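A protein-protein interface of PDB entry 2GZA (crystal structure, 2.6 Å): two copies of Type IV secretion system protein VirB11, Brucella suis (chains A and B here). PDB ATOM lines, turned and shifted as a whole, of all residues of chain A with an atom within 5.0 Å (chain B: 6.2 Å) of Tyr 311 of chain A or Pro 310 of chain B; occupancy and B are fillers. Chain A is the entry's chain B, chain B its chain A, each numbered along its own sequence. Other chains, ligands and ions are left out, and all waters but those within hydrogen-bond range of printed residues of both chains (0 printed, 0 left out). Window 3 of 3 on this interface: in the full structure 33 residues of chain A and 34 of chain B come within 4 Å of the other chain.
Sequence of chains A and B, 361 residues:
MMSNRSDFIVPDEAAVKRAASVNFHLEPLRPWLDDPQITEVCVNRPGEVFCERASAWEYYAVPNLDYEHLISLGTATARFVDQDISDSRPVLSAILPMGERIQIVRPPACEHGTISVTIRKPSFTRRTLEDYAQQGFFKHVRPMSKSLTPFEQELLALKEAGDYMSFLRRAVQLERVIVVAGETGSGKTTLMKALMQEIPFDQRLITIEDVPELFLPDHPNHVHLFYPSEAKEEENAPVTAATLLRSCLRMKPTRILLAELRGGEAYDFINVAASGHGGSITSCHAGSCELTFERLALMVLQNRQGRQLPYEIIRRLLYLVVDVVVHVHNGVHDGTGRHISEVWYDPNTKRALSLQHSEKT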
ATOM      1  N   GLU A 294     -19.950 -23.566 -23.112  1.00  0.00           N
ATOM      2  CA  GLU A 294     -21.398 -23.681 -23.109  1.00  0.00           C
ATOM      3  C   GLU A 294     -21.817 -25.140 -23.004  1.00  0.00           C
ATOM      4  O   GLU A 294     -22.672 -25.471 -22.181  1.00  0.00           O
ATOM      5  CB  GLU A 294     -21.961 -23.030 -24.360  1.00  0.00           C
ATOM      6  CG  GLU A 294     -23.269 -22.377 -24.142  1.00  0.00           C
ATOM      7  CD  GLU A 294     -23.187 -21.087 -23.337  1.00  0.00           C
ATOM      8  OE1 GLU A 294     -23.962 -20.944 -22.369  1.00  0.00           O
ATOM      9  OE2 GLU A 294     -22.370 -20.208 -23.674  1.00  0.00           O
ATOM     10  N   ALA A 297     -20.722 -26.887 -19.566  1.00  0.00           N
ATOM     11  CA  ALA A 297     -21.673 -26.564 -18.499  1.00  0.00           C
ATOM     12  C   ALA A 297     -22.882 -27.496 -18.510  1.00  0.00           C
ATOM     13  O   ALA A 297     -23.328 -27.948 -17.457  1.00  0.00           O
ATOM     14  CB  ALA A 297     -22.114 -25.101 -18.583  1.00  0.00           C
ATOM     15  N   LEU A 298     -23.396 -27.787 -19.702  1.00  0.00           N
ATOM     16  CA  LEU A 298     -24.515 -28.701 -19.868  1.00  0.00           C
ATOM     17  C   LEU A 298     -24.148 -30.101 -19.417  1.00  0.00           C
ATOM     18  O   LEU A 298     -24.973 -30.811 -18.863  1.00  0.00           O
ATOM     19  CB  LEU A 298     -24.958 -28.719 -21.330  1.00  0.00           C
ATOM     20  CG  LEU A 298     -25.978 -27.701 -21.844  1.00  0.00           C
ATOM     21  CD1 LEU A 298     -26.039 -26.421 -21.029  1.00  0.00           C
ATOM     22  CD2 LEU A 298     -25.722 -27.410 -23.325  1.00  0.00           C
ATOM     23  N   LEU A 301     -24.249 -30.320 -15.585  1.00  0.00           N
ATOM     24  CA  LEU A 301     -25.628 -30.437 -15.128  1.00  0.00           C
ATOM     25  C   LEU A 301     -26.202 -31.850 -15.229  1.00  0.00           C
ATOM     26  O   LEU A 301     -27.301 -32.112 -14.744  1.00  0.00           O
ATOM     27  CB  LEU A 301     -26.514 -29.433 -15.865  1.00  0.00           C
ATOM     28  CG  LEU A 301     -26.236 -27.959 -15.561  1.00  0.00           C
ATOM     29  CD1 LEU A 301     -26.939 -27.076 -16.566  1.00  0.00           C
ATOM     30  CD2 LEU A 301     -26.649 -27.593 -14.142  1.00  0.00           C
ATOM     31  N   LEU A 309     -25.226 -27.040  -8.382  1.00  0.00           N
ATOM     32  CA  LEU A 309     -24.486 -25.826  -8.600  1.00  0.00           C
ATOM     33  C   LEU A 309     -25.288 -24.860  -9.446  1.00  0.00           C
ATOM     34  O   LEU A 309     -25.805 -25.235 -10.499  1.00  0.00           O
ATOM     35  CB  LEU A 309     -23.152 -26.138  -9.276  1.00  0.00           C
ATOM     36  CG  LEU A 309     -22.188 -27.058  -8.528  1.00  0.00           C
ATOM     37  CD1 LEU A 309     -21.012 -27.410  -9.425  1.00  0.00           C
ATOM     38  CD2 LEU A 309     -21.707 -26.428  -7.221  1.00  0.00           C
ATOM     39  N   PRO A 310     -25.397 -23.605  -8.984  1.00  0.00           N
ATOM     40  CA  PRO A 310     -25.950 -22.560  -9.835  1.00  0.00           C
ATOM     41  C   PRO A 310     -25.138 -22.477 -11.128  1.00  0.00           C
ATOM     42  O   PRO A 310     -23.930 -22.742 -11.123  1.00  0.00           O
ATOM     43  CB  PRO A 310     -25.756 -21.293  -8.995  1.00  0.00           C
ATOM     44  CG  PRO A 310     -25.716 -21.778  -7.582  1.00  0.00           C
ATOM     45  CD  PRO A 310     -25.008 -23.098  -7.657  1.00  0.00           C
ATOM     46  N   TYR A 311     -25.798 -22.127 -12.224  1.00  0.00           N
ATOM     47  CA  TYR A 311     -25.134 -22.080 -13.515  1.00  0.00           C
ATOM     48  C   TYR A 311     -23.905 -21.167 -13.494  1.00  0.00           C
ATOM     49  O   TYR A 311     -22.867 -21.510 -14.068  1.00  0.00           O
ATOM     50  CB  TYR A 311     -26.110 -21.679 -14.619  1.00  0.00           C
ATOM     51  CG  TYR A 311     -25.490 -21.647 -15.999  1.00  0.00           C
ATOM     52  CD1 TYR A 311     -25.405 -22.797 -16.778  1.00  0.00           C
ATOM     53  CD2 TYR A 311     -24.977 -20.467 -16.516  1.00  0.00           C
ATOM     54  CE1 TYR A 311     -24.832 -22.765 -18.043  1.00  0.00           C
ATOM     55  CE2 TYR A 311     -24.407 -20.428 -17.769  1.00  0.00           C
ATOM     56  CZ  TYR A 311     -24.330 -21.576 -18.529  1.00  0.00           C
ATOM     57  OH  TYR A 311     -23.749 -21.508 -19.777  1.00  0.00           O
ATOM     58  N   GLU A 312     -24.013 -20.022 -12.820  1.00  0.00           N
ATOM     59  CA  GLU A 312     -22.906 -19.059 -12.753  1.00  0.00           C
ATOM     60  C   GLU A 312     -21.668 -19.674 -12.080  1.00  0.00           C
ATOM     61  O   GLU A 312     -20.527 -19.383 -12.458  1.00  0.00           O
ATOM     62  CB  GLU A 312     -23.340 -17.760 -12.053  1.00  0.00           C
ATOM     63  CG  GLU A 312     -23.240 -17.774 -10.518  1.00  0.00           C
ATOM     64  CD  GLU A 312     -24.302 -16.922  -9.817  1.00  0.00           C
ATOM     65  OE1 GLU A 312     -25.487 -17.335  -9.763  1.00  0.00           O
ATOM     66  OE2 GLU A 312     -23.942 -15.844  -9.298  1.00  0.00           O
ATOM     67  N   ILE A 313     -21.921 -20.542 -11.102  1.00  0.00           N
ATOM     68  CA  ILE A 313     -20.874 -21.238 -10.376  1.00  0.00           C
ATOM     69  C   ILE A 313     -20.205 -22.313 -11.258  1.00  0.00           C
ATOM     70  O   ILE A 313     -18.994 -22.500 -11.203  1.00  0.00           O
ATOM     71  CB  ILE A 313     -21.418 -21.834  -9.027  1.00  0.00           C
ATOM     72  CG1 ILE A 313     -21.988 -20.741  -8.104  1.00  0.00           C
ATOM     73  CG2 ILE A 313     -20.371 -22.656  -8.290  1.00  0.00           C
ATOM     74  CD1 ILE A 313     -21.008 -19.639  -7.727  1.00  0.00           C
ATOM     75  N   ILE A 314     -20.991 -23.009 -12.070  1.00  0.00           N
ATOM     76  CA  ILE A 314     -20.440 -23.960 -13.037  1.00  0.00           C
ATOM     77  C   ILE A 314     -19.526 -23.242 -14.040  1.00  0.00           C
ATOM     78  O   ILE A 314     -18.384 -23.659 -14.254  1.00  0.00           O
ATOM     79  CB  ILE A 314     -21.550 -24.739 -13.768  1.00  0.00           C
ATOM     80  CG1 ILE A 314     -22.287 -25.638 -12.778  1.00  0.00           C
ATOM     81  CG2 ILE A 314     -20.964 -25.569 -14.930  1.00  0.00           C
ATOM     82  CD1 ILE A 314     -23.588 -26.169 -13.287  1.00  0.00           C
ATOM     83  N   ARG A 315     -20.027 -22.153 -14.623  1.00  0.00           N
ATOM     84  CA  ARG A 315     -19.257 -21.344 -15.563  1.00  0.00           C
ATOM     85  C   ARG A 315     -17.985 -20.797 -14.930  1.00  0.00           C
ATOM     86  O   ARG A 315     -16.949 -20.684 -15.594  1.00  0.00           O
ATOM     87  CB  ARG A 315     -20.099 -20.196 -16.127  1.00  0.00           C
ATOM     88  CG  ARG A 315     -21.178 -20.637 -17.107  1.00  0.00           C
ATOM     89  CD  ARG A 315     -20.621 -21.494 -18.254  1.00  0.00           C
ATOM     90  NE  ARG A 315     -19.718 -20.734 -19.108  1.00  0.00           N
ATOM     91  CZ  ARG A 315     -20.067 -20.132 -20.240  1.00  0.00           C
ATOM     92  NH1 ARG A 315     -21.311 -20.204 -20.703  1.00  0.00           N
ATOM     93  NH2 ARG A 315     -19.155 -19.464 -20.918  1.00  0.00           N
ATOM     94  N   ARG A 316     -18.062 -20.467 -13.646  1.00  0.00           N
ATOM     95  CA  ARG A 316     -16.896 -19.987 -12.926  1.00  0.00           C
ATOM     96  C   ARG A 316     -15.879 -21.106 -12.668  1.00  0.00           C
ATOM     97  O   ARG A 316     -14.667 -20.884 -12.734  1.00  0.00           O
ATOM     98  CB  ARG A 316     -17.308 -19.343 -11.607  1.00  0.00           C
ATOM     99  CG  ARG A 316     -16.158 -18.665 -10.913  1.00  0.00           C
ATOM    100  CD  ARG A 316     -15.945 -19.267  -9.558  1.00  0.00           C
ATOM    101  NE  ARG A 316     -16.689 -18.556  -8.530  1.00  0.00           N
ATOM    102  CZ  ARG A 316     -16.119 -17.906  -7.526  1.00  0.00           C
ATOM    103  NH1 ARG A 316     -14.803 -17.883  -7.421  1.00  0.00           N
ATOM    104  NH2 ARG A 316     -16.855 -17.279  -6.625  1.00  0.00           N
ATOM    105  N   GLY B 306     -32.652 -28.521 -18.938  1.00  0.00           N
ATOM    106  CA  GLY B 306     -33.065 -27.193 -19.376  1.00  0.00           C
ATOM    107  C   GLY B 306     -33.575 -26.336 -18.236  1.00  0.00           C
ATOM    108  O   GLY B 306     -33.350 -25.133 -18.212  1.00  0.00           O
ATOM    109  N   ARG B 307     -34.252 -26.973 -17.287  1.00  0.00           N
ATOM    110  CA  ARG B 307     -34.756 -26.316 -16.072  1.00  0.00           C
ATOM    111  C   ARG B 307     -33.689 -25.719 -15.159  1.00  0.00           C
ATOM    112  O   ARG B 307     -33.980 -24.799 -14.400  1.00  0.00           O
ATOM    113  CB  ARG B 307     -35.614 -27.281 -15.262  1.00  0.00           C
ATOM    114  CG  ARG B 307     -37.093 -27.019 -15.335  1.00  0.00           C
ATOM    115  CD  ARG B 307     -37.891 -28.209 -14.817  1.00  0.00           C
ATOM    116  NE  ARG B 307     -38.153 -29.180 -15.879  1.00  0.00           N
ATOM    117  CZ  ARG B 307     -38.922 -30.255 -15.752  1.00  0.00           C
ATOM    118  NH1 ARG B 307     -39.524 -30.523 -14.598  1.00  0.00           N
ATOM    119  NH2 ARG B 307     -39.093 -31.063 -16.786  1.00  0.00           N
ATOM    120  N   GLN B 308     -32.469 -26.248 -15.227  1.00  0.00           N
ATOM    121  CA  GLN B 308     -31.372 -25.789 -14.381  1.00  0.00           C
ATOM    122  C   GLN B 308     -30.786 -24.477 -14.872  1.00  0.00           C
ATOM    123  O   GLN B 308     -30.127 -23.761 -14.109  1.00  0.00           O
ATOM    124  CB  GLN B 308     -30.263 -26.832 -14.347  1.00  0.00           C
ATOM    125  CG  GLN B 308     -30.731 -28.267 -14.436  1.00  0.00           C
ATOM    126  CD  GLN B 308     -31.334 -28.781 -13.152  1.00  0.00           C
ATOM    127  OE1 GLN B 308     -31.617 -28.018 -12.217  1.00  0.00           O
ATOM    128  NE2 GLN B 308     -31.529 -30.094 -13.090  1.00  0.00           N
ATOM    129  N   LEU B 309     -31.014 -24.183 -16.150  1.00  0.00           N
ATOM    130  CA  LEU B 309     -30.481 -22.990 -16.778  1.00  0.00           C
ATOM    131  C   LEU B 309     -31.318 -21.778 -16.407  1.00  0.00           C
ATOM    132  O   LEU B 309     -32.543 -21.811 -16.526  1.00  0.00           O
ATOM    133  CB  LEU B 309     -30.440 -23.150 -18.308  1.00  0.00           C
ATOM    134  CG  LEU B 309     -29.674 -24.340 -18.889  1.00  0.00           C
ATOM    135  CD1 LEU B 309     -29.971 -24.492 -20.363  1.00  0.00           C
ATOM    136  CD2 LEU B 309     -28.180 -24.206 -18.655  1.00  0.00           C
ATOM    137  N   PRO B 310     -30.662 -20.706 -15.938  1.00  0.00           N
ATOM    138  CA  PRO B 310     -31.367 -19.441 -15.803  1.00  0.00           C
ATOM    139  C   PRO B 310     -31.954 -19.040 -17.155  1.00  0.00           C
ATOM    140  O   PRO B 310     -31.392 -19.367 -18.213  1.00  0.00           O
ATOM    141  CB  PRO B 310     -30.270 -18.473 -15.381  1.00  0.00           C
ATOM    142  CG  PRO B 310     -29.249 -19.341 -14.707  1.00  0.00           C
ATOM    143  CD  PRO B 310     -29.261 -20.609 -15.498  1.00  0.00           C
ATOM    144  N   TYR B 311     -33.090 -18.358 -17.114  1.00  0.00           N
ATOM    145  CA  TYR B 311     -33.786 -17.981 -18.330  1.00  0.00           C
ATOM    146  C   TYR B 311     -32.900 -17.198 -19.311  1.00  0.00           C
ATOM    147  O   TYR B 311     -32.956 -17.424 -20.525  1.00  0.00           O
ATOM    148  CB  TYR B 311     -35.066 -17.213 -17.994  1.00  0.00           C
ATOM    149  CG  TYR B 311     -35.860 -16.849 -19.214  1.00  0.00           C
ATOM    150  CD1 TYR B 311     -36.742 -17.767 -19.800  1.00  0.00           C
ATOM    151  CD2 TYR B 311     -35.716 -15.602 -19.809  1.00  0.00           C
ATOM    152  CE1 TYR B 311     -37.470 -17.440 -20.933  1.00  0.00           C
ATOM    153  CE2 TYR B 311     -36.434 -15.268 -20.948  1.00  0.00           C
ATOM    154  CZ  TYR B 311     -37.307 -16.190 -21.504  1.00  0.00           C
ATOM    155  OH  TYR B 311     -38.008 -15.861 -22.636  1.00  0.00           O
ATOM    156  N   GLU B 312     -32.087 -16.290 -18.780  1.00  0.00           N
ATOM    157  CA  GLU B 312     -31.201 -15.474 -19.600  1.00  0.00           C
ATOM    158  C   GLU B 312     -30.177 -16.331 -20.345  1.00  0.00           C
ATOM    159  O   GLU B 312     -29.787 -16.016 -21.472  1.00  0.00           O
ATOM    160  CB  GLU B 312     -30.533 -14.365 -18.775  1.00  0.00           C
ATOM    161  CG  GLU B 312     -29.731 -14.834 -17.546  1.00  0.00           C
ATOM    162  CD  GLU B 312     -30.570 -15.009 -16.260  1.00  0.00           C
ATOM    163  OE1 GLU B 312     -31.806 -15.258 -16.332  1.00  0.00           O
ATOM    164  OE2 GLU B 312     -29.967 -14.909 -15.162  1.00  0.00           O
ATOM    165  N   ILE B 313     -29.774 -17.428 -19.717  1.00  0.00           N
ATOM    166  CA  ILE B 313     -28.818 -18.364 -20.304  1.00  0.00           C
ATOM    167  C   ILE B 313     -29.455 -19.154 -21.451  1.00  0.00           C
ATOM    168  O   ILE B 313     -28.823 -19.388 -22.496  1.00  0.00           O
ATOM    169  CB  ILE B 313     -28.232 -19.311 -19.225  1.00  0.00           C
ATOM    170  CG1 ILE B 313     -27.432 -18.519 -18.175  1.00  0.00           C
ATOM    171  CG2 ILE B 313     -27.393 -20.431 -19.864  1.00  0.00           C
ATOM    172  CD1 ILE B 313     -26.361 -17.561 -18.742  1.00  0.00           C
ATOM    173  N   ILE B 314     -30.704 -19.558 -21.253  1.00  0.00           N
ATOM    174  CA  ILE B 314     -31.450 -20.231 -22.300  1.00  0.00           C
ATOM    175  C   ILE B 314     -31.572 -19.335 -23.537  1.00  0.00           C
ATOM    176  O   ILE B 314     -31.281 -19.777 -24.653  1.00  0.00           O
ATOM    177  CB  ILE B 314     -32.848 -20.677 -21.833  1.00  0.00           C
ATOM    178  CG1 ILE B 314     -32.747 -21.754 -20.753  1.00  0.00           C
ATOM    179  CG2 ILE B 314     -33.656 -21.196 -23.018  1.00  0.00           C
ATOM    180  CD1 ILE B 314     -34.049 -21.990 -19.970  1.00  0.00           C
ATOM    181  N   ARG B 315     -31.985 -18.088 -23.322  1.00  0.00           N
ATOM    182  CA  ARG B 315     -32.106 -17.114 -24.402  1.00  0.00           C
ATOM    183  C   ARG B 315     -30.766 -16.844 -25.081  1.00  0.00           C
ATOM    184  O   ARG B 315     -30.717 -16.641 -26.290  1.00  0.00           O
ATOM    185  CB  ARG B 315     -32.740 -15.816 -23.901  1.00  0.00           C
ATOM    186  CG  ARG B 315     -34.206 -15.953 -23.455  1.00  0.00           C
ATOM    187  CD  ARG B 315     -35.139 -16.420 -24.580  1.00  0.00           C
ATOM    188  NE  ARG B 315     -35.158 -15.468 -25.680  1.00  0.00           N
ATOM    189  CZ  ARG B 315     -36.086 -14.540 -25.856  1.00  0.00           C
ATOM    190  NH1 ARG B 315     -37.113 -14.443 -25.014  1.00  0.00           N
ATOM    191  NH2 ARG B 315     -35.990 -13.714 -26.889  1.00  0.00           N
ATOM    192  N   ARG B 316     -29.683 -16.862 -24.314  1.00  0.00           N
ATOM    193  CA  ARG B 316     -28.361 -16.684 -24.887  1.00  0.00           C
ATOM    194  C   ARG B 316     -27.942 -17.896 -25.732  1.00  0.00           C
ATOM    195  O   ARG B 316     -27.300 -17.748 -26.779  1.00  0.00           O
ATOM    196  CB  ARG B 316     -27.343 -16.415 -23.795  1.00  0.00           C
ATOM    197  CG  ARG B 316     -25.998 -16.008 -24.337  1.00  0.00           C
ATOM    198  CD  ARG B 316     -24.954 -16.968 -23.869  1.00  0.00           C
ATOM    199  NE  ARG B 316     -24.365 -16.557 -22.605  1.00  0.00           N
ATOM    200  CZ  ARG B 316     -23.066 -16.337 -22.442  1.00  0.00           C
ATOM    201  NH1 ARG B 316     -22.230 -16.489 -23.460  1.00  0.00           N
ATOM    202  NH2 ARG B 316     -22.598 -15.968 -21.262  1.00  0.00           N
ATOM    203  N   LEU B 317     -28.308 -19.087 -25.276  1.00  0.00           N
ATOM    204  CA  LEU B 317     -28.041 -20.306 -26.025  1.00  0.00           C
ATOM    205  C   LEU B 317     -28.757 -20.340 -27.354  1.00  0.00           C
ATOM    206  O   LEU B 317     -28.187 -20.773 -28.357  1.00  0.00           O
ATOM    207  CB  LEU B 317     -28.430 -21.544 -25.224  1.00  0.00           C
ATOM    208  CG  LEU B 317     -27.292 -22.379 -24.655  1.00  0.00           C
ATOM    209  CD1 LEU B 317     -26.204 -22.590 -25.716  1.00  0.00           C
ATOM    210  CD2 LEU B 317     -26.726 -21.706 -23.426  1.00  0.00           C
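The guanidinium group (NH1) of Arg 316 of chain B lies within salt-bridge range of the side-chain carboxylate (OE2) of Glu 294 of chain A.
OH of Tyr 311 of chain A sits at hydrogen-bond distance from NH1 of Arg 315 of chain A.
The guanidinium group (NH1) of Arg 315 of chain A lies within salt-bridge range of the side-chain carboxylate (OE2) of Glu 294 of chain A.
The side-chain carboxylate of Glu 294 of chain A lies within hydrogen-bond range of the side-chain hydroxyl of Tyr 311 of chain A (2.7 Å).
Among the printed residues, pairs that only touch across the chains: Glu 294 of chain A with Leu 317 of chain B, Leu 298 of chain A with Leu 309 of chain B, Leu 301 of chain A with Gln 308 of chain B, Leu 301 of chain A with Leu 309 of chain B, Tyr 311 of chain A with Leu 309 of chain B, Tyr 311 of chain A with Pro 310 of chain B and Tyr 311 of chain A with Ile 313 of chain B.
Of the printed residues of chain B, Leu 298 of chain A touches Leu 309.
Of the printed residues of chain A, Ile 313 of chain B touches Tyr 311.
Of the printed residues of chain A, Leu 317 of chain B touches Glu 294.
The nearest residue of chain B that does not touch Tyr 311 of chain A is Gln 308 of chain B (4.6 Å).
The nearest printed residue of chain A that does not touch Gln 308 of chain B is Tyr 311 of chain A (4.6 Å).
Of the 12 printed residues of chain A, 4 touch a printed residue of chain B.
Printed residues of chain A that touch a printed residue of chain B: Glu 294, Leu 298, Leu 301 and Tyr 311.
Hydrophobic or aromatic side chains of chain A within 4 Å of the printed part of chain B: Leu 298, Leu 301 and Tyr 311.
Printed residues of chain B that touch a printed residue of chain A: Gln 308, Leu 309, Pro 310, Ile 313, Arg 316 and Leu 317.
Among the printed residues, 8 pairs touch across the chains.
Tyr 311 of chain A touches Leu 309 of chain B, but with the chains exchanged Leu 309 of chain A does not touch Tyr 311 of chain B (12.0 Å).
Tyr 311 of chain A touches Pro 310 of chain B, but with the chains exchanged Pro 310 of chain A does not touch Tyr 311 of chain B (10.8 Å).
Tyr 311 of chain A touches Ile 313 of chain B, but with the chains exchanged Ile 313 of chain A does not touch Tyr 311 of chain B (12.9 Å).
8 positions are printed for both chains.
Of the 8 pairs that touch across the chains among the printed residues, none has its exchanged pair printed and touching as well.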
